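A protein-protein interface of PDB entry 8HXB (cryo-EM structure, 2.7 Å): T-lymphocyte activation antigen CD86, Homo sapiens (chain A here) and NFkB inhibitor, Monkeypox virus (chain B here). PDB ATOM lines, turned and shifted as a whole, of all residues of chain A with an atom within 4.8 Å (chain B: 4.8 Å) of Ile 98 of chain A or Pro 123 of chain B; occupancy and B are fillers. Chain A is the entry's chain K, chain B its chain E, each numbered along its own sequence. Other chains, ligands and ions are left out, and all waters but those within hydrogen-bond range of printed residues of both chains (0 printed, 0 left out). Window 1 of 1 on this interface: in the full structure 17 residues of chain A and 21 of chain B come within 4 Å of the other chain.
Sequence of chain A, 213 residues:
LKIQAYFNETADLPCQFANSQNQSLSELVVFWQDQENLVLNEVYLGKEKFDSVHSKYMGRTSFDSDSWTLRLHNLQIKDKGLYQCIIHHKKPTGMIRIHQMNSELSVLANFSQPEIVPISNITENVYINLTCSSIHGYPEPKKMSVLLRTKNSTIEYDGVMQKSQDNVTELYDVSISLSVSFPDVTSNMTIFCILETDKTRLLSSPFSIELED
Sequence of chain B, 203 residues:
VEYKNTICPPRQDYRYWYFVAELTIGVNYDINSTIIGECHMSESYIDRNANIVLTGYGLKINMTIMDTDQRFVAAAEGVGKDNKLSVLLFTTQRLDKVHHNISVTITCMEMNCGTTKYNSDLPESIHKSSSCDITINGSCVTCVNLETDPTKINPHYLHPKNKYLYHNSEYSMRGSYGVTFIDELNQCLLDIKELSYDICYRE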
ATOM      1  N   PHE A  17     -25.690 -13.173 -25.757  1.00  0.00           N
ATOM      2  CA  PHE A  17     -24.271 -13.090 -26.072  1.00  0.00           C
ATOM      3  C   PHE A  17     -23.888 -11.620 -26.187  1.00  0.00           C
ATOM      4  O   PHE A  17     -24.490 -10.874 -26.965  1.00  0.00           O
ATOM      5  CB  PHE A  17     -23.978 -13.838 -27.372  1.00  0.00           C
ATOM      6  CG  PHE A  17     -22.512 -14.115 -27.623  1.00  0.00           C
ATOM      7  CD1 PHE A  17     -21.561 -13.963 -26.621  1.00  0.00           C
ATOM      8  CD2 PHE A  17     -22.091 -14.525 -28.876  1.00  0.00           C
ATOM      9  CE1 PHE A  17     -20.227 -14.216 -26.867  1.00  0.00           C
ATOM     10  CE2 PHE A  17     -20.757 -14.779 -29.126  1.00  0.00           C
ATOM     11  CZ  PHE A  17     -19.826 -14.624 -28.119  1.00  0.00           C
ATOM     12  N   GLN A  23     -17.496 -10.226 -33.405  1.00  0.00           N
ATOM     13  CA  GLN A  23     -17.395 -11.072 -34.579  1.00  0.00           C
ATOM     14  C   GLN A  23     -18.781 -11.406 -35.112  1.00  0.00           C
ATOM     15  O   GLN A  23     -19.775 -11.399 -34.381  1.00  0.00           O
ATOM     16  CB  GLN A  23     -16.602 -12.344 -34.272  1.00  0.00           C
ATOM     17  CG  GLN A  23     -17.398 -13.490 -33.710  1.00  0.00           C
ATOM     18  CD  GLN A  23     -16.609 -14.281 -32.701  1.00  0.00           C
ATOM     19  OE1 GLN A  23     -15.423 -14.036 -32.492  1.00  0.00           O
ATOM     20  NE2 GLN A  23     -17.260 -15.242 -32.075  1.00  0.00           N
ATOM     21  N   LEU A  28     -19.857 -19.001 -36.684  1.00  0.00           N
ATOM     22  CA  LEU A  28     -20.341 -19.184 -35.320  1.00  0.00           C
ATOM     23  C   LEU A  28     -21.338 -20.328 -35.321  1.00  0.00           C
ATOM     24  O   LEU A  28     -22.326 -20.277 -36.057  1.00  0.00           O
ATOM     25  CB  LEU A  28     -21.030 -17.920 -34.791  1.00  0.00           C
ATOM     26  CG  LEU A  28     -20.245 -16.897 -33.976  1.00  0.00           C
ATOM     27  CD1 LEU A  28     -21.047 -15.630 -33.756  1.00  0.00           C
ATOM     28  CD2 LEU A  28     -19.828 -17.493 -32.685  1.00  0.00           C
ATOM     29  N   ILE A  87     -22.795 -21.587 -27.683  1.00  0.00           N
ATOM     30  CA  ILE A  87     -22.264 -20.865 -28.824  1.00  0.00           C
ATOM     31  C   ILE A  87     -20.805 -21.267 -28.944  1.00  0.00           C
ATOM     32  O   ILE A  87     -19.990 -20.939 -28.067  1.00  0.00           O
ATOM     33  CB  ILE A  87     -22.388 -19.345 -28.658  1.00  0.00           C
ATOM     34  CG1 ILE A  87     -23.809 -18.944 -28.281  1.00  0.00           C
ATOM     35  CG2 ILE A  87     -21.987 -18.646 -29.922  1.00  0.00           C
ATOM     36  CD1 ILE A  87     -24.841 -19.367 -29.220  1.00  0.00           C
ATOM     37  N   HIS A  88     -20.481 -21.990 -30.008  1.00  0.00           N
ATOM     38  CA  HIS A  88     -19.121 -22.316 -30.392  1.00  0.00           C
ATOM     39  C   HIS A  88     -18.643 -21.333 -31.449  1.00  0.00           C
ATOM     40  O   HIS A  88     -19.442 -20.752 -32.187  1.00  0.00           O
ATOM     41  CB  HIS A  88     -19.022 -23.731 -30.960  1.00  0.00           C
ATOM     42  CG  HIS A  88     -19.262 -24.816 -29.960  1.00  0.00           C
ATOM     43  ND1 HIS A  88     -20.453 -24.966 -29.289  1.00  0.00           N
ATOM     44  CD2 HIS A  88     -18.460 -25.817 -29.530  1.00  0.00           C
ATOM     45  CE1 HIS A  88     -20.374 -26.011 -28.486  1.00  0.00           C
ATOM     46  NE2 HIS A  88     -19.173 -26.544 -28.611  1.00  0.00           N
ATOM     47  N   HIS A  89     -17.333 -21.158 -31.523  1.00  0.00           N
ATOM     48  CA  HIS A  89     -16.707 -20.356 -32.567  1.00  0.00           C
ATOM     49  C   HIS A  89     -15.932 -21.312 -33.458  1.00  0.00           C
ATOM     50  O   HIS A  89     -14.870 -21.807 -33.068  1.00  0.00           O
ATOM     51  CB  HIS A  89     -15.799 -19.286 -31.973  1.00  0.00           C
ATOM     52  CG  HIS A  89     -14.883 -18.648 -32.967  1.00  0.00           C
ATOM     53  ND1 HIS A  89     -13.514 -18.776 -32.906  1.00  0.00           N
ATOM     54  CD2 HIS A  89     -15.140 -17.867 -34.041  1.00  0.00           C
ATOM     55  CE1 HIS A  89     -12.967 -18.104 -33.902  1.00  0.00           C
ATOM     56  NE2 HIS A  89     -13.932 -17.544 -34.607  1.00  0.00           N
ATOM     57  N   ILE A  96     -14.185 -24.060 -30.981  1.00  0.00           N
ATOM     58  CA  ILE A  96     -14.015 -23.642 -29.593  1.00  0.00           C
ATOM     59  C   ILE A  96     -15.338 -23.109 -29.076  1.00  0.00           C
ATOM     60  O   ILE A  96     -15.915 -22.195 -29.674  1.00  0.00           O
ATOM     61  CB  ILE A  96     -12.932 -22.560 -29.462  1.00  0.00           C
ATOM     62  CG1 ILE A  96     -11.596 -23.039 -30.022  1.00  0.00           C
ATOM     63  CG2 ILE A  96     -12.794 -22.126 -28.028  1.00  0.00           C
ATOM     64  CD1 ILE A  96     -10.497 -22.012 -29.886  1.00  0.00           C
ATOM     65  N   ARG A  97     -15.808 -23.658 -27.958  1.00  0.00           N
ATOM     66  CA  ARG A  97     -16.970 -23.089 -27.293  1.00  0.00           C
ATOM     67  C   ARG A  97     -16.593 -21.757 -26.663  1.00  0.00           C
ATOM     68  O   ARG A  97     -15.658 -21.686 -25.862  1.00  0.00           O
ATOM     69  CB  ARG A  97     -17.496 -24.030 -26.214  1.00  0.00           C
ATOM     70  CG  ARG A  97     -18.492 -23.342 -25.315  1.00  0.00           C
ATOM     71  CD  ARG A  97     -19.242 -24.267 -24.406  1.00  0.00           C
ATOM     72  NE  ARG A  97     -18.399 -24.962 -23.453  1.00  0.00           N
ATOM     73  CZ  ARG A  97     -18.262 -26.275 -23.398  1.00  0.00           C
ATOM     74  NH1 ARG A  97     -18.876 -27.069 -24.255  1.00  0.00           N
ATOM     75  NH2 ARG A  97     -17.503 -26.801 -22.447  1.00  0.00           N
ATOM     76  N   ILE A  98     -17.319 -20.698 -27.013  1.00  0.00           N
ATOM     77  CA  ILE A  98     -17.033 -19.389 -26.460  1.00  0.00           C
ATOM     78  C   ILE A  98     -18.091 -18.934 -25.462  1.00  0.00           C
ATOM     79  O   ILE A  98     -17.759 -18.185 -24.538  1.00  0.00           O
ATOM     80  CB  ILE A  98     -16.853 -18.327 -27.560  1.00  0.00           C
ATOM     81  CG1 ILE A  98     -17.942 -18.456 -28.603  1.00  0.00           C
ATOM     82  CG2 ILE A  98     -15.508 -18.493 -28.244  1.00  0.00           C
ATOM     83  CD1 ILE A  98     -17.894 -17.367 -29.581  1.00  0.00           C
ATOM     84  N   HIS A  99     -19.348 -19.354 -25.604  1.00  0.00           N
ATOM     85  CA  HIS A  99     -20.348 -18.864 -24.662  1.00  0.00           C
ATOM     86  C   HIS A  99     -21.322 -19.991 -24.372  1.00  0.00           C
ATOM     87  O   HIS A  99     -21.576 -20.834 -25.233  1.00  0.00           O
ATOM     88  CB  HIS A  99     -21.045 -17.594 -25.212  1.00  0.00           C
ATOM     89  CG  HIS A  99     -22.452 -17.352 -24.725  1.00  0.00           C
ATOM     90  ND1 HIS A  99     -23.483 -18.204 -25.047  1.00  0.00           N
ATOM     91  CD2 HIS A  99     -22.975 -16.462 -23.845  1.00  0.00           C
ATOM     92  CE1 HIS A  99     -24.595 -17.797 -24.465  1.00  0.00           C
ATOM     93  NE2 HIS A  99     -24.314 -16.739 -23.728  1.00  0.00           N
ATOM     94  N   GLN A 100     -21.837 -20.022 -23.152  1.00  0.00           N
ATOM     95  CA  GLN A 100     -22.959 -20.877 -22.811  1.00  0.00           C
ATOM     96  C   GLN A 100     -23.806 -20.140 -21.786  1.00  0.00           C
ATOM     97  O   GLN A 100     -23.298 -19.290 -21.053  1.00  0.00           O
ATOM     98  CB  GLN A 100     -22.474 -22.241 -22.311  1.00  0.00           C
ATOM     99  CG  GLN A 100     -22.438 -22.421 -20.823  1.00  0.00           C
ATOM    100  CD  GLN A 100     -22.378 -23.870 -20.424  1.00  0.00           C
ATOM    101  OE1 GLN A 100     -21.479 -24.598 -20.832  1.00  0.00           O
ATOM    102  NE2 GLN A 100     -23.328 -24.297 -19.608  1.00  0.00           N
ATOM    103  N   ASP B 121      -6.278 -20.855 -26.583  1.00  0.00           N
ATOM    104  CA  ASP B 121      -6.810 -20.380 -25.312  1.00  0.00           C
ATOM    105  C   ASP B 121      -8.328 -20.449 -25.390  1.00  0.00           C
ATOM    106  O   ASP B 121      -8.960 -19.618 -26.050  1.00  0.00           O
ATOM    107  CB  ASP B 121      -6.340 -18.962 -25.006  1.00  0.00           C
ATOM    108  CG  ASP B 121      -4.830 -18.832 -25.027  1.00  0.00           C
ATOM    109  OD1 ASP B 121      -4.136 -19.833 -24.747  1.00  0.00           O
ATOM    110  OD2 ASP B 121      -4.334 -17.726 -25.325  1.00  0.00           O
ATOM    111  N   LEU B 122      -8.908 -21.428 -24.708  1.00  0.00           N
ATOM    112  CA  LEU B 122     -10.346 -21.602 -24.695  1.00  0.00           C
ATOM    113  C   LEU B 122     -10.948 -20.621 -23.707  1.00  0.00           C
ATOM    114  O   LEU B 122     -10.543 -20.613 -22.537  1.00  0.00           O
ATOM    115  CB  LEU B 122     -10.716 -23.017 -24.299  1.00  0.00           C
ATOM    116  CG  LEU B 122      -9.983 -24.161 -24.992  1.00  0.00           C
ATOM    117  CD1 LEU B 122     -10.308 -25.477 -24.319  1.00  0.00           C
ATOM    118  CD2 LEU B 122     -10.321 -24.206 -26.457  1.00  0.00           C
ATOM    119  N   PRO B 123     -11.879 -19.775 -24.120  1.00  0.00           N
ATOM    120  CA  PRO B 123     -12.496 -18.850 -23.176  1.00  0.00           C
ATOM    121  C   PRO B 123     -13.492 -19.562 -22.283  1.00  0.00           C
ATOM    122  O   PRO B 123     -14.086 -20.579 -22.647  1.00  0.00           O
ATOM    123  CB  PRO B 123     -13.188 -17.839 -24.091  1.00  0.00           C
ATOM    124  CG  PRO B 123     -13.580 -18.648 -25.250  1.00  0.00           C
ATOM    125  CD  PRO B 123     -12.456 -19.629 -25.465  1.00  0.00           C
ATOM    126  N   GLU B 124     -13.645 -19.027 -21.080  1.00  0.00           N
ATOM    127  CA  GLU B 124     -14.618 -19.578 -20.155  1.00  0.00           C
ATOM    128  C   GLU B 124     -16.024 -19.215 -20.621  1.00  0.00           C
ATOM    129  O   GLU B 124     -16.315 -18.049 -20.911  1.00  0.00           O
ATOM    130  CB  GLU B 124     -14.347 -19.052 -18.756  1.00  0.00           C
ATOM    131  CG  GLU B 124     -15.421 -19.344 -17.765  1.00  0.00           C
ATOM    132  CD  GLU B 124     -14.991 -19.023 -16.353  1.00  0.00           C
ATOM    133  OE1 GLU B 124     -14.271 -18.019 -16.170  1.00  0.00           O
ATOM    134  OE2 GLU B 124     -15.376 -19.766 -15.428  1.00  0.00           O
ATOM    135  N   SER B 125     -16.892 -20.226 -20.707  1.00  0.00           N
ATOM    136  CA  SER B 125     -18.187 -20.065 -21.363  1.00  0.00           C
ATOM    137  C   SER B 125     -19.139 -19.202 -20.546  1.00  0.00           C
ATOM    138  O   SER B 125     -19.827 -18.334 -21.096  1.00  0.00           O
ATOM    139  CB  SER B 125     -18.800 -21.435 -21.609  1.00  0.00           C
ATOM    140  OG  SER B 125     -17.938 -22.208 -22.416  1.00  0.00           O
ATOM    141  N   LYS B 128     -17.105 -15.518 -18.342  1.00  0.00           N
ATOM    142  CA  LYS B 128     -15.906 -15.157 -19.106  1.00  0.00           C
ATOM    143  C   LYS B 128     -14.778 -14.537 -18.289  1.00  0.00           C
ATOM    144  O   LYS B 128     -14.145 -13.576 -18.733  1.00  0.00           O
ATOM    145  CB  LYS B 128     -16.239 -14.182 -20.244  1.00  0.00           C
ATOM    146  CG  LYS B 128     -16.975 -14.729 -21.479  1.00  0.00           C
ATOM    147  CD  LYS B 128     -18.444 -15.020 -21.249  1.00  0.00           C
ATOM    148  CE  LYS B 128     -19.210 -15.126 -22.537  1.00  0.00           C
ATOM    149  NZ  LYS B 128     -20.600 -15.517 -22.227  1.00  0.00           N
ATOM    150  N   SER B 130     -12.064 -16.364 -16.816  1.00  0.00           N
ATOM    151  CA  SER B 130     -10.804 -17.084 -16.889  1.00  0.00           C
ATOM    152  C   SER B 130     -10.574 -17.593 -18.308  1.00  0.00           C
ATOM    153  O   SER B 130     -11.329 -17.290 -19.234  1.00  0.00           O
ATOM    154  CB  SER B 130     -10.792 -18.231 -15.881  1.00  0.00           C
ATOM    155  OG  SER B 130     -11.846 -19.139 -16.137  1.00  0.00           O
ATOM    156  N   TYR B 177     -15.265 -24.997 -20.273  1.00  0.00           N
ATOM    157  CA  TYR B 177     -14.350 -24.872 -21.392  1.00  0.00           C
ATOM    158  C   TYR B 177     -14.564 -26.070 -22.296  1.00  0.00           C
ATOM    159  O   TYR B 177     -14.727 -27.191 -21.814  1.00  0.00           O
ATOM    160  CB  TYR B 177     -12.896 -24.832 -20.938  1.00  0.00           C
ATOM    161  CG  TYR B 177     -12.612 -23.938 -19.755  1.00  0.00           C
ATOM    162  CD1 TYR B 177     -12.329 -22.595 -19.931  1.00  0.00           C
ATOM    163  CD2 TYR B 177     -12.602 -24.445 -18.465  1.00  0.00           C
ATOM    164  CE1 TYR B 177     -12.052 -21.783 -18.859  1.00  0.00           C
ATOM    165  CE2 TYR B 177     -12.332 -23.636 -17.387  1.00  0.00           C
ATOM    166  CZ  TYR B 177     -12.061 -22.307 -17.591  1.00  0.00           C
ATOM    167  OH  TYR B 177     -11.789 -21.492 -16.520  1.00  0.00           O
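Gln 23 of chain A touches none of the printed residues of chain B. His 89 of chain A touches none of the printed residues of chain B. Of chain B, only Pro 123, Glu 124, Ser 125 and Lys 128 come within 4 Å of Ile 98 of chain A. Of the printed residues of chain B, Gln 100 of chain A touches Ser 125. Of the printed residues of chain A, Pro 123 of chain B touches Ile 96, Arg 97 and Ile 98. Of the printed residues of chain A, Tyr 177 of chain B touches Arg 97 (2.9 Å). The nearest printed residue of chain A that does not touch Pro 123 of chain B is His 99 of chain A (5.8 Å).
Of the 11 printed residues of chain A, 5 touch a printed residue of chain B. Printed residues of chain A that touch a printed residue of chain B: Ile 96, Arg 97, Ile 98, His 99 and Gln 100. Along chain A the printed residues that touch a printed residue of chain B span positions 96 to 100. Hydrophobic or aromatic side chains of chain B that line the printed part of chain A: Leu 122 and Pro 123. Among the printed residues, no Asp or Glu carboxylate lies within 4 Å of a Lys or Arg side-chain nitrogen of the other chain.
OG of Ser 130 of chain B is in hydrogen-bond range of OE1 of Glu 124 of chain B (2.7 Å). The backbone carbonyl oxygen (O) of Ser 125 of chain B is in hydrogen-bond range of the side-chain amino group (NZ) of Lys 128 of chain B (3.1 Å). The backbone carbonyl oxygen (O) of Ile 87 of chain A lies within hydrogen-bond range of the backbone NH (N) of Ile 98 of chain A. The backbone carbonyl oxygen of His 99 of chain A is in hydrogen-bond range of the backbone NH of Ile 87 of chain A (2.8 Å). The backbone NH of His 89 of chain A is in hydrogen-bond range of the backbone carbonyl oxygen of Ile 96 of chain A (2.6 Å).
The side-chain hydroxyl (OG) of Ser 125 of chain B is in hydrogen-bond range of the guanidinium group (NE) of Arg 97 of chain A, 3.0 Å away. The backbone carbonyl oxygen (O) of Ser 125 of chain B is in hydrogen-bond range of the backbone NH (N) of Gln 100 of chain A. The guanidinium group (NH2) of Arg 97 of chain A lies within hydrogen-bond range of the backbone carbonyl oxygen (O) of Tyr 177 of chain B, at 2.9 Å.
Among the printed residues, merely in contact across the chains: Ile 96 of chain A with Leu 122 of chain B, Ile 96 of chain A with Pro 123 of chain B, Arg 97 of chain A with Pro 123 of chain B, Ile 98 of chain A with Pro 123 of chain B, Ile 98 of chain A with Glu 124 of chain B, Ile 98 of chain A with Ser 125 of chain B, Ile 98 of chain A with Lys 128 of chain B, His 99 of chain A with Ser 125 of chain B and His 99 of chain A with Lys 128 of chain B.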
